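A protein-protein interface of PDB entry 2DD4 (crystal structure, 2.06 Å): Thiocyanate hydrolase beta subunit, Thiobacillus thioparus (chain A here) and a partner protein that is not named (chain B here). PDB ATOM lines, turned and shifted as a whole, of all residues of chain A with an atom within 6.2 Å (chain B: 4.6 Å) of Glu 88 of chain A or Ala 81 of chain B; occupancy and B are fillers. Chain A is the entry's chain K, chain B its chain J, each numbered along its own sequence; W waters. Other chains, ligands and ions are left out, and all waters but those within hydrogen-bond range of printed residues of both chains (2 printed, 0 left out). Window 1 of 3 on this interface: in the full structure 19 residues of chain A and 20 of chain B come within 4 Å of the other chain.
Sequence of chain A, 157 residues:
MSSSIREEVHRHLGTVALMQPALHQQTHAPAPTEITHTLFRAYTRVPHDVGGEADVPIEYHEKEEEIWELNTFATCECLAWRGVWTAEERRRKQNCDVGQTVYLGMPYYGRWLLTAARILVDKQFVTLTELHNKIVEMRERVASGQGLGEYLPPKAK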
ATOM      1  N   THR A  86      21.112  -9.292  25.030  1.00  0.00           N
ATOM      2  CA  THR A  86      21.912  -9.284  23.812  1.00  0.00           C
ATOM      3  C   THR A  86      21.612  -7.921  23.192  1.00  0.00           C
ATOM      4  O   THR A  86      20.625  -7.278  23.558  1.00  0.00           O
ATOM      5  CB  THR A  86      21.499 -10.393  22.816  1.00  0.00           C
ATOM      6  OG1 THR A  86      20.111 -10.258  22.489  1.00  0.00           O
ATOM      7  CG2 THR A  86      21.766 -11.776  23.403  1.00  0.00           C
ATOM      8  N   ALA A  87      22.453  -7.475  22.267  1.00  0.00           N
ATOM      9  CA  ALA A  87      22.244  -6.176  21.637  1.00  0.00           C
ATOM     10  C   ALA A  87      20.877  -6.096  20.962  1.00  0.00           C
ATOM     11  O   ALA A  87      20.217  -5.058  21.004  1.00  0.00           O
ATOM     12  CB  ALA A  87      23.356  -5.900  20.620  1.00  0.00           C
ATOM     13  N   GLU A  88      20.444  -7.190  20.342  1.00  0.00           N
ATOM     14  CA  GLU A  88      19.149  -7.179  19.675  1.00  0.00           C
ATOM     15  C   GLU A  88      17.995  -6.944  20.640  1.00  0.00           C
ATOM     16  O   GLU A  88      17.045  -6.237  20.308  1.00  0.00           O
ATOM     17  CB  GLU A  88      18.936  -8.469  18.879  1.00  0.00           C
ATOM     18  CG  GLU A  88      19.325  -8.300  17.418  1.00  0.00           C
ATOM     19  CD  GLU A  88      18.603  -7.122  16.780  1.00  0.00           C
ATOM     20  OE1 GLU A  88      19.276  -6.210  16.249  1.00  0.00           O
ATOM     21  OE2 GLU A  88      17.355  -7.108  16.817  1.00  0.00           O
ATOM     22  N   GLU A  89      18.067  -7.532  21.831  1.00  0.00           N
ATOM     23  CA  GLU A  89      17.016  -7.310  22.815  1.00  0.00           C
ATOM     24  C   GLU A  89      17.011  -5.821  23.158  1.00  0.00           C
ATOM     25  O   GLU A  89      15.950  -5.222  23.331  1.00  0.00           O
ATOM     26  CB  GLU A  89      17.263  -8.141  24.076  1.00  0.00           C
ATOM     27  CG  GLU A  89      17.100  -9.640  23.850  1.00  0.00           C
ATOM     28  CD  GLU A  89      17.384 -10.465  25.093  1.00  0.00           C
ATOM     29  OE1 GLU A  89      18.534 -10.439  25.585  1.00  0.00           O
ATOM     30  OE2 GLU A  89      16.454 -11.145  25.573  1.00  0.00           O
ATOM     31  N   ARG A  90      18.200  -5.224  23.246  1.00  0.00           N
ATOM     32  CA  ARG A  90      18.303  -3.798  23.552  1.00  0.00           C
ATOM     33  C   ARG A  90      17.663  -2.943  22.462  1.00  0.00           C
ATOM     34  O   ARG A  90      16.875  -2.048  22.759  1.00  0.00           O
ATOM     35  CB  ARG A  90      19.767  -3.369  23.728  1.00  0.00           C
ATOM     36  CG  ARG A  90      19.932  -1.847  23.908  1.00  0.00           C
ATOM     37  CD  ARG A  90      21.350  -1.444  24.327  1.00  0.00           C
ATOM     38  NE  ARG A  90      22.363  -1.679  23.296  1.00  0.00           N
ATOM     39  CZ  ARG A  90      22.419  -1.044  22.127  1.00  0.00           C
ATOM     40  NH1 ARG A  90      21.512  -0.123  21.821  1.00  0.00           N
ATOM     41  NH2 ARG A  90      23.391  -1.324  21.262  1.00  0.00           N
ATOM     42  N   ARG A  91      18.003  -3.214  21.202  1.00  0.00           N
ATOM     43  CA  ARG A  91      17.441  -2.443  20.092  1.00  0.00           C
ATOM     44  C   ARG A  91      15.924  -2.505  20.094  1.00  0.00           C
ATOM     45  O   ARG A  91      15.254  -1.481  19.958  1.00  0.00           O
ATOM     46  CB  ARG A  91      17.973  -2.951  18.746  1.00  0.00           C
ATOM     47  CG  ARG A  91      19.473  -2.740  18.561  1.00  0.00           C
ATOM     48  CD  ARG A  91      19.913  -2.905  17.105  1.00  0.00           C
ATOM     49  NE  ARG A  91      21.371  -2.825  17.018  1.00  0.00           N
ATOM     50  CZ  ARG A  91      22.192  -3.843  17.258  1.00  0.00           C
ATOM     51  NH1 ARG A  91      21.706  -5.036  17.581  1.00  0.00           N
ATOM     52  NH2 ARG A  91      23.506  -3.654  17.231  1.00  0.00           N
ATOM     53  N   ARG A  92      15.380  -3.707  20.249  1.00  0.00           N
ATOM     54  CA  ARG A  92      13.932  -3.877  20.272  1.00  0.00           C
ATOM     55  C   ARG A  92      13.294  -3.074  21.406  1.00  0.00           C
ATOM     56  O   ARG A  92      12.290  -2.400  21.203  1.00  0.00           O
ATOM     57  CB  ARG A  92      13.581  -5.364  20.405  1.00  0.00           C
ATOM     58  CG  ARG A  92      12.085  -5.656  20.495  1.00  0.00           C
ATOM     59  CD  ARG A  92      11.615  -5.704  21.939  1.00  0.00           C
ATOM     60  NE  ARG A  92      12.178  -6.846  22.654  1.00  0.00           N
ATOM     61  CZ  ARG A  92      11.905  -7.141  23.923  1.00  0.00           C
ATOM     62  NH1 ARG A  92      11.074  -6.373  24.621  1.00  0.00           N
ATOM     63  NH2 ARG A  92      12.453  -8.210  24.492  1.00  0.00           N
ATOM     64  N   LYS A  93      13.876  -3.134  22.600  1.00  0.00           N
ATOM     65  CA  LYS A  93      13.325  -2.399  23.738  1.00  0.00           C
ATOM     66  C   LYS A  93      13.576  -0.890  23.659  1.00  0.00           C
ATOM     67  O   LYS A  93      12.717  -0.082  24.019  1.00  0.00           O
ATOM     68  CB  LYS A  93      13.927  -2.914  25.053  1.00  0.00           C
ATOM     69  CG  LYS A  93      13.618  -4.371  25.376  1.00  0.00           C
ATOM     70  CD  LYS A  93      14.344  -4.815  26.646  1.00  0.00           C
ATOM     71  CE  LYS A  93      13.791  -4.128  27.891  1.00  0.00           C
ATOM     72  NZ  LYS A  93      12.385  -4.559  28.176  1.00  0.00           N
ATOM     73  N   TYR B  53       8.042  -6.121  16.261  1.00  0.00           N
ATOM     74  CA  TYR B  53       9.436  -6.008  15.839  1.00  0.00           C
ATOM     75  C   TYR B  53       9.754  -6.624  14.486  1.00  0.00           C
ATOM     76  O   TYR B  53       9.145  -7.611  14.073  1.00  0.00           O
ATOM     77  CB  TYR B  53      10.355  -6.647  16.891  1.00  0.00           C
ATOM     78  CG  TYR B  53      11.818  -6.244  16.780  1.00  0.00           C
ATOM     79  CD1 TYR B  53      12.207  -4.914  16.943  1.00  0.00           C
ATOM     80  CD2 TYR B  53      12.812  -7.194  16.533  1.00  0.00           C
ATOM     81  CE1 TYR B  53      13.545  -4.536  16.866  1.00  0.00           C
ATOM     82  CE2 TYR B  53      14.157  -6.829  16.452  1.00  0.00           C
ATOM     83  CZ  TYR B  53      14.514  -5.496  16.621  1.00  0.00           C
ATOM     84  OH  TYR B  53      15.833  -5.116  16.555  1.00  0.00           O
ATOM     85  N   ARG B  55      13.326  -6.233  11.346  1.00  0.00           N
ATOM     86  CA  ARG B  55      14.498  -5.498  10.884  1.00  0.00           C
ATOM     87  C   ARG B  55      14.544  -5.530   9.362  1.00  0.00           C
ATOM     88  O   ARG B  55      15.578  -5.275   8.741  1.00  0.00           O
ATOM     89  CB  ARG B  55      15.786  -6.055  11.497  1.00  0.00           C
ATOM     90  CG  ARG B  55      15.874  -5.833  13.007  1.00  0.00           C
ATOM     91  CD  ARG B  55      17.288  -6.028  13.528  1.00  0.00           C
ATOM     92  NE  ARG B  55      18.171  -4.928  13.147  1.00  0.00           N
ATOM     93  CZ  ARG B  55      18.170  -3.728  13.723  1.00  0.00           C
ATOM     94  NH1 ARG B  55      17.332  -3.459  14.718  1.00  0.00           N
ATOM     95  NH2 ARG B  55      19.016  -2.793  13.303  1.00  0.00           N
ATOM     96  N   ALA B  77      16.435 -11.635  13.812  1.00  0.00           N
ATOM     97  CA  ALA B  77      16.337 -10.623  14.865  1.00  0.00           C
ATOM     98  C   ALA B  77      14.965 -10.680  15.526  1.00  0.00           C
ATOM     99  O   ALA B  77      14.823 -10.384  16.713  1.00  0.00           O
ATOM    100  CB  ALA B  77      16.575  -9.239  14.291  1.00  0.00           C
ATOM    101  N   ASP B  79      13.504 -13.094  16.451  1.00  0.00           N
ATOM    102  CA  ASP B  79      13.555 -14.094  17.513  1.00  0.00           C
ATOM    103  C   ASP B  79      14.598 -13.739  18.566  1.00  0.00           C
ATOM    104  O   ASP B  79      14.342 -13.823  19.765  1.00  0.00           O
ATOM    105  CB  ASP B  79      13.867 -15.483  16.946  1.00  0.00           C
ATOM    106  CG  ASP B  79      12.698 -16.081  16.192  1.00  0.00           C
ATOM    107  OD1 ASP B  79      11.545 -15.871  16.630  1.00  0.00           O
ATOM    108  OD2 ASP B  79      12.928 -16.773  15.175  1.00  0.00           O
ATOM    109  N   GLU B  80      15.776 -13.338  18.106  1.00  0.00           N
ATOM    110  CA  GLU B  80      16.867 -12.980  19.002  1.00  0.00           C
ATOM    111  C   GLU B  80      16.491 -11.845  19.965  1.00  0.00           C
ATOM    112  O   GLU B  80      16.839 -11.888  21.147  1.00  0.00           O
ATOM    113  CB  GLU B  80      18.090 -12.586  18.166  1.00  0.00           C
ATOM    114  CG  GLU B  80      19.413 -12.569  18.919  1.00  0.00           C
ATOM    115  CD  GLU B  80      20.603 -12.437  17.973  1.00  0.00           C
ATOM    116  OE1 GLU B  80      20.712 -11.398  17.289  1.00  0.00           O
ATOM    117  OE2 GLU B  80      21.422 -13.378  17.910  1.00  0.00           O
ATOM    118  N   ALA B  81      15.764 -10.849  19.465  1.00  0.00           N
ATOM    119  CA  ALA B  81      15.359  -9.700  20.277  1.00  0.00           C
ATOM    120  C   ALA B  81      14.382 -10.057  21.400  1.00  0.00           C
ATOM    121  O   ALA B  81      14.104  -9.231  22.276  1.00  0.00           O
ATOM    122  CB  ALA B  81      14.749  -8.621  19.384  1.00  0.00           C
ATOM    123  N   PHE B  82      13.859 -11.279  21.372  1.00  0.00           N
ATOM    124  CA  PHE B  82      12.938 -11.727  22.407  1.00  0.00           C
ATOM    125  C   PHE B  82      13.492 -12.930  23.168  1.00  0.00           C
ATOM    126  O   PHE B  82      12.759 -13.648  23.854  1.00  0.00           O
ATOM    127  CB  PHE B  82      11.565 -12.023  21.792  1.00  0.00           C
ATOM    128  CG  PHE B  82      10.772 -10.777  21.481  1.00  0.00           C
ATOM    129  CD1 PHE B  82      10.108 -10.089  22.496  1.00  0.00           C
ATOM    130  CD2 PHE B  82      10.738 -10.258  20.188  1.00  0.00           C
ATOM    131  CE1 PHE B  82       9.423  -8.899  22.229  1.00  0.00           C
ATOM    132  CE2 PHE B  82      10.060  -9.073  19.909  1.00  0.00           C
ATOM    133  CZ  PHE B  82       9.401  -8.389  20.930  1.00  0.00           C
ATOM    134  N   GLY B  83      14.803 -13.129  23.044  1.00  0.00           N
ATOM    135  CA  GLY B  83      15.475 -14.214  23.741  1.00  0.00           C
ATOM    136  C   GLY B  83      15.280 -15.603  23.168  1.00  0.00           C
ATOM    137  O   GLY B  83      15.511 -16.594  23.862  1.00  0.00           O
HETATM  138  O   HOH W   1      22.000  -9.664  19.057  1.00  0.00           O
HETATM  139  O   HOH W   2      18.925 -13.049  22.528  1.00  0.00           O
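The side-chain hydroxyl (OH) of Tyr 53 of chain B sits at hydrogen-bond distance from the side-chain carboxylate (OE2) of Glu 88 of chain A, 2.5 Å away.
The guanidinium group (NH2) of Arg 92 of chain A lies within hydrogen-bond range of the backbone carbonyl oxygen (O) of Ala 81 of chain B (2.9 Å).
OE1 of Glu 88 of chain A is in salt-bridge range of NE of Arg 55 of chain B, at 3.5 Å.
The guanidinium group (NH1) of Arg 55 of chain B sits at hydrogen-bond distance from the side-chain hydroxyl (OH) of Tyr 53 of chain B (2.9 Å).
N of Thr 86 of chain A is in hydrogen-bond range of OE1 of Glu 89 of chain A, 2.9 Å away.
The guanidinium group (NH1) of Arg 91 of chain A is in salt-bridge range of the side-chain carboxylate (OE1) of Glu 88 of chain A, 3.0 Å away.
Among the printed residues, pairs that only touch across the chains: Thr 86 of chain A with Glu 80 of chain B, Glu 88 of chain A with Ala 77 of chain B, Glu 88 of chain A with Glu 80 of chain B, Glu 88 of chain A with Ala 81 of chain B, Glu 89 of chain A with Glu 80 of chain B, Glu 89 of chain A with Ala 81 of chain B, Glu 89 of chain A with Gly 83 of chain B, Arg 91 of chain A with Tyr 53 of chain B, Arg 91 of chain A with Arg 55 of chain B, Arg 92 of chain A with Tyr 53 of chain B and Arg 92 of chain A with Phe 82 of chain B.
Of chain B, only Tyr 53, Arg 55, Ala 77, Glu 80 and Ala 81 come within 4 Å of Glu 88 of chain A.
Printed residues of chain B within 4 Å of Glu 89 of chain A: Glu 80, Ala 81 and Gly 83.
Of the printed residues of chain A, Arg 55 of chain B touches Glu 88 and Arg 91.
Printed residues of chain A within 4 Å of Glu 80 of chain B: Thr 86, Glu 88 and Glu 89.
Of chain A, only Glu 88 (3.4 Å), Glu 89 (3.4 Å) and Arg 92 (2.9 Å) come within 4 Å of Ala 81 of chain B.
Of the printed residues of chain A, Gly 83 of chain B touches Glu 89.
The nearest printed residue of chain B that does not touch Glu 88 of chain A is Phe 82 of chain B (6.0 Å).
The nearest residue of chain A that does not touch Ala 81 of chain B is Thr 86 of chain A (5.3 Å).
The nearest printed residue of chain B that does not touch Thr 86 of chain A is Ala 81 of chain B (5.3 Å).
Of the 8 printed residues of chain B, 7 touch a printed residue of chain A.
Hydrophobic or aromatic side chains of chain B within 4 Å of the printed part of chain A: Tyr 53, Ala 77, Ala 81 and Phe 82.
Of the 8 printed residues of chain A, 5 touch a printed residue of chain B.
Along chain A the printed residues that touch a printed residue of chain B span positions 86 to 92.
Among the printed residues, Asp or Glu carboxylates within 4 Å of a Lys or Arg side-chain nitrogen of the other chain: Glu 88 of chain A with Arg 55 of chain B (3.5 Å).
Water W2 lies within hydrogen-bond range of O of Glu 80 of chain B and OG1 of Thr 86 of chain A.
Water W1 bridges OE1 of Glu 80 of chain B (2.8 Å) and N of Glu 88 of chain A (3.2 Å).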
